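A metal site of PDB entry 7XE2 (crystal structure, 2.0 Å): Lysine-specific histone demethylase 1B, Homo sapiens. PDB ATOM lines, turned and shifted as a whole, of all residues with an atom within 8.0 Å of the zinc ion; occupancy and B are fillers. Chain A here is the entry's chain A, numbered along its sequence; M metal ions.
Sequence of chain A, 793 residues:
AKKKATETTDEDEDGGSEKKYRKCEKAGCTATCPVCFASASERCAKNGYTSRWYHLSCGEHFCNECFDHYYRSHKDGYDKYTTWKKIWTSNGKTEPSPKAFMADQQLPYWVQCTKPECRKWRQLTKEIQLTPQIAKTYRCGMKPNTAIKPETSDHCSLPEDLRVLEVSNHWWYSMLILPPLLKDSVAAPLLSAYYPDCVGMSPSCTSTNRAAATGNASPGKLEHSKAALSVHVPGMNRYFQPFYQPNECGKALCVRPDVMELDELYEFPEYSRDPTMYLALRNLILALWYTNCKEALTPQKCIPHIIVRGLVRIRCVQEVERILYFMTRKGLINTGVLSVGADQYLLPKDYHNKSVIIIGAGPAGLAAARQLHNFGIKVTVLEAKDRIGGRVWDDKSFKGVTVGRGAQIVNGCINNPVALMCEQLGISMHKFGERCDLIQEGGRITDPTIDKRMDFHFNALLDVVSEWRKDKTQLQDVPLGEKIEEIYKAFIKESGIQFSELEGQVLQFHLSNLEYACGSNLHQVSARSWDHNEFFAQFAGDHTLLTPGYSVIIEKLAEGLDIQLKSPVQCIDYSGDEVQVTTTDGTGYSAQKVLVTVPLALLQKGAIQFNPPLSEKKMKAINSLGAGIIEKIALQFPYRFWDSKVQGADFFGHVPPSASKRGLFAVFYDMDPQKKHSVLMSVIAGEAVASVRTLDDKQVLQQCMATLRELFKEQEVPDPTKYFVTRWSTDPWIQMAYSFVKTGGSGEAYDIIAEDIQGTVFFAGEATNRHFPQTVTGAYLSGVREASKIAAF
The side-chain sulfur (SG) of Cys 66 lies close to the backbone NH (N) of Ala 40 (3.4 Å). The side-chain sulfur (SG) of Cys 66 sits close to the backbone NH (N) of Ser 41, 3.6 Å away. The side-chain sulfur (SG) of Cys 63 sits close to the backbone NH (N) of Ala 45 (3.4 Å). The backbone NH (N) of Glu 65 sits close to the side-chain sulfur (SG) of Cys 63 (3.7 Å). The side-chain sulfur (SG) of Cys 44 lies close to the backbone NH (N) of Lys 46, 3.3 Å away. N of Ser 39 sits close to SG of Cys 36. The backbone NH of Cys 36 sits at hydrogen-bond distance from the backbone carbonyl oxygen of Lys 46 (2.7 Å). SG of Cys 36 sits close to N of Ala 38, at 3.4 Å.
Residues that only touch the zinc ion: Ala 45 (3.98 Å) and Ser 39 (3.998 Å). Of the 24 residues printed, 6 come within 4 Å of the zinc ion. The nearest printed residue that does not touch the zinc ion is Lys 46 (4.6 Å).
The zinc ion is bound by the side-chain sulfur (SG) of Cys 66 (2.3 Å). The zinc ion is bound by SG of Cys 63. The zinc ion is bound by SG of Cys 44 (2.3 Å). The zinc ion is bound by SG of Cys 36, at 2.4 Å.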
ATOM      1  N   VAL A  35      24.864   5.986 -20.279  1.00  0.00           N
ATOM      2  CA  VAL A  35      23.442   6.206 -20.469  1.00  0.00           C
ATOM      3  C   VAL A  35      23.271   7.599 -21.050  1.00  0.00           C
ATOM      4  O   VAL A  35      24.099   8.473 -20.802  1.00  0.00           O
ATOM      5  CB  VAL A  35      22.660   6.059 -19.154  1.00  0.00           C
ATOM      6  CG1 VAL A  35      22.832   4.679 -18.608  1.00  0.00           C
ATOM      7  CG2 VAL A  35      23.149   7.108 -18.153  1.00  0.00           C
ATOM      8  N   CYS A  36      22.202   7.808 -21.815  1.00  0.00           N
ATOM      9  CA  CYS A  36      22.003   9.131 -22.412  1.00  0.00           C
ATOM     10  C   CYS A  36      21.299  10.039 -21.423  1.00  0.00           C
ATOM     11  O   CYS A  36      20.216   9.705 -20.930  1.00  0.00           O
ATOM     12  CB  CYS A  36      21.207   9.034 -23.707  1.00  0.00           C
ATOM     13  SG  CYS A  36      21.212  10.607 -24.574  1.00  0.00           S
ATOM     14  N   PHE A  37      21.902  11.194 -21.122  1.00  0.00           N
ATOM     15  CA  PHE A  37      21.232  12.197 -20.296  1.00  0.00           C
ATOM     16  C   PHE A  37      20.241  13.044 -21.085  1.00  0.00           C
ATOM     17  O   PHE A  37      19.410  13.720 -20.462  1.00  0.00           O
ATOM     18  CB  PHE A  37      22.244  13.150 -19.633  1.00  0.00           C
ATOM     19  CG  PHE A  37      22.999  14.010 -20.617  1.00  0.00           C
ATOM     20  CD1 PHE A  37      22.410  15.121 -21.197  1.00  0.00           C
ATOM     21  CD2 PHE A  37      24.320  13.723 -20.942  1.00  0.00           C
ATOM     22  CE1 PHE A  37      23.091  15.903 -22.119  1.00  0.00           C
ATOM     23  CE2 PHE A  37      25.020  14.504 -21.838  1.00  0.00           C
ATOM     24  CZ  PHE A  37      24.408  15.595 -22.438  1.00  0.00           C
ATOM     25  N   ALA A  38      20.331  13.083 -22.404  1.00  0.00           N
ATOM     26  CA  ALA A  38      19.535  14.051 -23.150  1.00  0.00           C
ATOM     27  C   ALA A  38      18.104  13.565 -23.311  1.00  0.00           C
ATOM     28  O   ALA A  38      17.156  14.309 -23.037  1.00  0.00           O
ATOM     29  CB  ALA A  38      20.160  14.329 -24.514  1.00  0.00           C
ATOM     30  N   SER A  39      17.944  12.303 -23.736  1.00  0.00           N
ATOM     31  CA  SER A  39      16.668  11.710 -24.118  1.00  0.00           C
ATOM     32  C   SER A  39      15.796  12.725 -24.840  1.00  0.00           C
ATOM     33  O   SER A  39      14.669  13.012 -24.460  1.00  0.00           O
ATOM     34  CB  SER A  39      15.944  11.103 -22.923  1.00  0.00           C
ATOM     35  OG  SER A  39      15.576  12.106 -22.003  1.00  0.00           O
ATOM     36  N   ALA A  40      16.394  13.325 -25.879  1.00  0.00           N
ATOM     37  CA  ALA A  40      15.720  14.324 -26.706  1.00  0.00           C
ATOM     38  C   ALA A  40      15.033  13.699 -27.905  1.00  0.00           C
ATOM     39  O   ALA A  40      13.927  14.093 -28.267  1.00  0.00           O
ATOM     40  CB  ALA A  40      16.736  15.367 -27.171  1.00  0.00           C
ATOM     41  N   SER A  41      15.671  12.705 -28.516  1.00  0.00           N
ATOM     42  CA  SER A  41      15.088  12.008 -29.659  1.00  0.00           C
ATOM     43  C   SER A  41      14.086  10.966 -29.196  1.00  0.00           C
ATOM     44  O   SER A  41      14.198  10.409 -28.096  1.00  0.00           O
ATOM     45  CB  SER A  41      16.178  11.348 -30.502  1.00  0.00           C
ATOM     46  OG  SER A  41      15.677  10.872 -31.748  1.00  0.00           O
ATOM     47  N   GLU A  42      13.081  10.722 -30.038  1.00  0.00           N
ATOM     48  CA  GLU A  42      12.188   9.594 -29.816  1.00  0.00           C
ATOM     49  C   GLU A  42      12.921   8.257 -29.925  1.00  0.00           C
ATOM     50  O   GLU A  42      12.455   7.261 -29.365  1.00  0.00           O
ATOM     51  CB  GLU A  42      11.025   9.631 -30.817  1.00  0.00           C
ATOM     52  CG  GLU A  42      10.205  10.884 -30.694  1.00  0.00           C
ATOM     53  CD  GLU A  42       9.861  11.199 -29.260  1.00  0.00           C
ATOM     54  OE1 GLU A  42       8.942  10.534 -28.721  1.00  0.00           O
ATOM     55  OE2 GLU A  42      10.530  12.078 -28.655  1.00  0.00           O
ATOM     56  N   ARG A  43      14.049   8.230 -30.635  1.00  0.00           N
ATOM     57  CA  ARG A  43      14.849   7.019 -30.780  1.00  0.00           C
ATOM     58  C   ARG A  43      16.091   7.035 -29.902  1.00  0.00           C
ATOM     59  O   ARG A  43      17.066   6.345 -30.212  1.00  0.00           O
ATOM     60  CB  ARG A  43      15.239   6.838 -32.253  1.00  0.00           C
ATOM     61  CG  ARG A  43      14.038   6.736 -33.160  1.00  0.00           C
ATOM     62  CD  ARG A  43      14.424   6.431 -34.599  1.00  0.00           C
ATOM     63  NE  ARG A  43      13.232   6.107 -35.375  1.00  0.00           N
ATOM     64  CZ  ARG A  43      13.223   5.830 -36.676  1.00  0.00           C
ATOM     65  NH1 ARG A  43      14.342   5.833 -37.390  1.00  0.00           N
ATOM     66  NH2 ARG A  43      12.079   5.551 -37.276  1.00  0.00           N
ATOM     67  N   CYS A  44      16.069   7.811 -28.806  1.00  0.00           N
ATOM     68  CA  CYS A  44      17.189   7.869 -27.875  1.00  0.00           C
ATOM     69  C   CYS A  44      17.587   6.465 -27.440  1.00  0.00           C
ATOM     70  O   CYS A  44      16.740   5.663 -27.025  1.00  0.00           O
ATOM     71  CB  CYS A  44      16.832   8.715 -26.654  1.00  0.00           C
ATOM     72  SG  CYS A  44      18.047   8.663 -25.245  1.00  0.00           S
ATOM     73  N   ALA A  45      18.883   6.166 -27.524  1.00  0.00           N
ATOM     74  CA  ALA A  45      19.337   4.822 -27.179  1.00  0.00           C
ATOM     75  C   ALA A  45      19.243   4.526 -25.679  1.00  0.00           C
ATOM     76  O   ALA A  45      19.446   3.372 -25.285  1.00  0.00           O
ATOM     77  CB  ALA A  45      20.772   4.613 -27.674  1.00  0.00           C
ATOM     78  N   LYS A  46      18.940   5.529 -24.849  1.00  0.00           N
ATOM     79  CA  LYS A  46      18.673   5.316 -23.429  1.00  0.00           C
ATOM     80  C   LYS A  46      19.906   4.783 -22.703  1.00  0.00           C
ATOM     81  O   LYS A  46      20.789   5.565 -22.313  1.00  0.00           O
ATOM     82  CB  LYS A  46      17.488   4.363 -23.238  1.00  0.00           C
ATOM     83  CG  LYS A  46      16.136   5.026 -23.415  1.00  0.00           C
ATOM     84  CD  LYS A  46      16.005   6.235 -22.487  1.00  0.00           C
ATOM     85  CE  LYS A  46      14.632   6.899 -22.568  1.00  0.00           C
ATOM     86  NZ  LYS A  46      14.427   7.678 -23.835  1.00  0.00           N
ATOM     87  N   ASN A  47      19.979   3.461 -22.496  1.00  0.00           N
ATOM     88  CA  ASN A  47      21.143   2.844 -21.867  1.00  0.00           C
ATOM     89  C   ASN A  47      21.724   1.707 -22.696  1.00  0.00           C
ATOM     90  O   ASN A  47      22.546   0.951 -22.182  1.00  0.00           O
ATOM     91  CB  ASN A  47      20.807   2.348 -20.452  1.00  0.00           C
ATOM     92  CG  ASN A  47      19.653   1.362 -20.441  1.00  0.00           C
ATOM     93  OD1 ASN A  47      19.116   0.987 -21.478  1.00  0.00           O
ATOM     94  ND2 ASN A  47      19.288   0.924 -19.240  1.00  0.00           N
ATOM     95  N   THR A  50      24.225   2.289 -29.537  1.00  0.00           N
ATOM     96  CA  THR A  50      24.083   3.402 -30.462  1.00  0.00           C
ATOM     97  C   THR A  50      25.307   3.415 -31.372  1.00  0.00           C
ATOM     98  O   THR A  50      26.333   2.813 -31.064  1.00  0.00           O
ATOM     99  CB  THR A  50      23.937   4.749 -29.729  1.00  0.00           C
ATOM    100  OG1 THR A  50      23.749   5.802 -30.681  1.00  0.00           O
ATOM    101  CG2 THR A  50      25.174   5.040 -28.899  1.00  0.00           C
ATOM    102  N   TRP A  53      28.554   6.685 -28.762  1.00  0.00           N
ATOM    103  CA  TRP A  53      28.291   7.296 -27.461  1.00  0.00           C
ATOM    104  C   TRP A  53      29.204   8.523 -27.311  1.00  0.00           C
ATOM    105  O   TRP A  53      30.426   8.384 -27.184  1.00  0.00           O
ATOM    106  CB  TRP A  53      28.520   6.298 -26.324  1.00  0.00           C
ATOM    107  CG  TRP A  53      27.331   5.424 -26.003  1.00  0.00           C
ATOM    108  CD1 TRP A  53      27.224   4.074 -26.214  1.00  0.00           C
ATOM    109  CD2 TRP A  53      26.094   5.842 -25.429  1.00  0.00           C
ATOM    110  NE1 TRP A  53      25.974   3.633 -25.804  1.00  0.00           N
ATOM    111  CE2 TRP A  53      25.269   4.706 -25.319  1.00  0.00           C
ATOM    112  CE3 TRP A  53      25.587   7.077 -25.006  1.00  0.00           C
ATOM    113  CZ2 TRP A  53      23.976   4.755 -24.789  1.00  0.00           C
ATOM    114  CZ3 TRP A  53      24.308   7.136 -24.477  1.00  0.00           C
ATOM    115  CH2 TRP A  53      23.511   5.981 -24.373  1.00  0.00           C
ATOM    116  N   HIS A  61      27.125  11.172 -20.994  1.00  0.00           N
ATOM    117  CA  HIS A  61      27.200  10.765 -22.384  1.00  0.00           C
ATOM    118  C   HIS A  61      25.854  11.017 -23.036  1.00  0.00           C
ATOM    119  O   HIS A  61      24.826  11.100 -22.359  1.00  0.00           O
ATOM    120  CB  HIS A  61      27.612   9.271 -22.519  1.00  0.00           C
ATOM    121  CG  HIS A  61      28.898   8.943 -21.821  1.00  0.00           C
ATOM    122  ND1 HIS A  61      28.964   8.694 -20.472  1.00  0.00           N
ATOM    123  CD2 HIS A  61      30.175   8.857 -22.280  1.00  0.00           C
ATOM    124  CE1 HIS A  61      30.219   8.476 -20.119  1.00  0.00           C
ATOM    125  NE2 HIS A  61      30.981   8.572 -21.205  1.00  0.00           N
ATOM    126  N   PHE A  62      25.861  11.164 -24.354  1.00  0.00           N
ATOM    127  CA  PHE A  62      24.609  11.196 -25.097  1.00  0.00           C
ATOM    128  C   PHE A  62      24.757  10.412 -26.402  1.00  0.00           C
ATOM    129  O   PHE A  62      25.844  10.321 -26.975  1.00  0.00           O
ATOM    130  CB  PHE A  62      24.110  12.641 -25.341  1.00  0.00           C
ATOM    131  CG  PHE A  62      25.045  13.519 -26.130  1.00  0.00           C
ATOM    132  CD1 PHE A  62      26.105  14.186 -25.513  1.00  0.00           C
ATOM    133  CD2 PHE A  62      24.836  13.724 -27.488  1.00  0.00           C
ATOM    134  CE1 PHE A  62      26.950  15.007 -26.249  1.00  0.00           C
ATOM    135  CE2 PHE A  62      25.673  14.545 -28.230  1.00  0.00           C
ATOM    136  CZ  PHE A  62      26.725  15.182 -27.621  1.00  0.00           C
ATOM    137  N   CYS A  63      23.644   9.818 -26.839  1.00  0.00           N
ATOM    138  CA  CYS A  63      23.637   8.871 -27.939  1.00  0.00           C
ATOM    139  C   CYS A  63      23.637   9.603 -29.286  1.00  0.00           C
ATOM    140  O   CYS A  63      23.337  10.798 -29.374  1.00  0.00           O
ATOM    141  CB  CYS A  63      22.422   7.956 -27.840  1.00  0.00           C
ATOM    142  SG  CYS A  63      20.853   8.861 -28.099  1.00  0.00           S
ATOM    143  N   ASN A  64      23.943   8.851 -30.348  1.00  0.00           N
ATOM    144  CA  ASN A  64      24.002   9.481 -31.663  1.00  0.00           C
ATOM    145  C   ASN A  64      22.621   9.947 -32.119  1.00  0.00           C
ATOM    146  O   ASN A  64      22.518  10.905 -32.884  1.00  0.00           O
ATOM    147  CB  ASN A  64      24.587   8.514 -32.695  1.00  0.00           C
ATOM    148  CG  ASN A  64      24.848   9.201 -34.031  1.00  0.00           C
ATOM    149  OD1 ASN A  64      25.698  10.097 -34.136  1.00  0.00           O
ATOM    150  ND2 ASN A  64      24.093   8.810 -35.055  1.00  0.00           N
ATOM    151  N   GLU A  65      21.566   9.286 -31.665  1.00  0.00           N
ATOM    152  CA  GLU A  65      20.237   9.708 -32.075  1.00  0.00           C
ATOM    153  C   GLU A  65      19.913  11.095 -31.503  1.00  0.00           C
ATOM    154  O   GLU A  65      19.332  11.934 -32.194  1.00  0.00           O
ATOM    155  CB  GLU A  65      19.199   8.660 -31.664  1.00  0.00           C
ATOM    156  CG  GLU A  65      19.237   7.328 -32.487  1.00  0.00           C
ATOM    157  CD  GLU A  65      20.416   6.403 -32.116  1.00  0.00           C
ATOM    158  OE1 GLU A  65      21.199   6.744 -31.201  1.00  0.00           O
ATOM    159  OE2 GLU A  65      20.549   5.316 -32.733  1.00  0.00           O
ATOM    160  N   CYS A  66      20.336  11.358 -30.263  1.00  0.00           N
ATOM    161  CA  CYS A  66      20.111  12.689 -29.712  1.00  0.00           C
ATOM    162  C   CYS A  66      21.083  13.709 -30.273  1.00  0.00           C
ATOM    163  O   CYS A  66      20.720  14.886 -30.410  1.00  0.00           O
ATOM    164  CB  CYS A  66      20.190  12.656 -28.182  1.00  0.00           C
ATOM    165  SG  CYS A  66      18.886  11.658 -27.401  1.00  0.00           S
ATOM    166  N   PHE A  67      22.308  13.299 -30.607  1.00  0.00           N
ATOM    167  CA  PHE A  67      23.210  14.156 -31.386  1.00  0.00           C
ATOM    168  C   PHE A  67      22.515  14.651 -32.654  1.00  0.00           C
ATOM    169  O   PHE A  67      22.433  15.866 -32.905  1.00  0.00           O
ATOM    170  CB  PHE A  67      24.472  13.366 -31.721  1.00  0.00           C
ATOM    171  CG  PHE A  67      25.512  14.136 -32.508  1.00  0.00           C
ATOM    172  CD1 PHE A  67      25.364  14.324 -33.885  1.00  0.00           C
ATOM    173  CD2 PHE A  67      26.665  14.595 -31.895  1.00  0.00           C
ATOM    174  CE1 PHE A  67      26.318  15.016 -34.606  1.00  0.00           C
ATOM    175  CE2 PHE A  67      27.633  15.277 -32.620  1.00  0.00           C
ATOM    176  CZ  PHE A  67      27.451  15.483 -33.982  1.00  0.00           C
ATOM    177  N   HIS A  69      19.363  14.621 -33.382  1.00  0.00           N
ATOM    178  CA  HIS A  69      18.144  15.373 -33.056  1.00  0.00           C
ATOM    179  C   HIS A  69      18.366  16.875 -33.167  1.00  0.00           C
ATOM    180  O   HIS A  69      17.497  17.609 -33.669  1.00  0.00           O
ATOM    181  CB  HIS A  69      17.673  15.005 -31.652  1.00  0.00           C
ATOM    182  CG  HIS A  69      16.506  15.805 -31.172  1.00  0.00           C
ATOM    183  ND1 HIS A  69      15.208  15.533 -31.560  1.00  0.00           N
ATOM    184  CD2 HIS A  69      16.429  16.864 -30.345  1.00  0.00           C
ATOM    185  CE1 HIS A  69      14.389  16.395 -30.995  1.00  0.00           C
ATOM    186  NE2 HIS A  69      15.104  17.222 -30.251  1.00  0.00           N
ATOM    187  N   MET A 102      25.107  20.723 -25.692  1.00  0.00           N
ATOM    188  CA  MET A 102      24.612  19.870 -24.605  1.00  0.00           C
ATOM    189  C   MET A 102      25.072  20.385 -23.249  1.00  0.00           C
ATOM    190  O   MET A 102      24.272  20.461 -22.308  1.00  0.00           O
ATOM    191  CB  MET A 102      25.078  18.423 -24.796  1.00  0.00           C
ATOM    192  CG  MET A 102      24.429  17.666 -25.969  1.00  0.00           C
ATOM    193  SD  MET A 102      22.629  17.544 -25.823  1.00  0.00           S
ATOM    194  CE  MET A 102      22.248  16.221 -26.987  1.00  0.00           C
HETATM  195 ZN    ZN M   1      19.771   9.848 -26.309  1.00  0.00          ZN
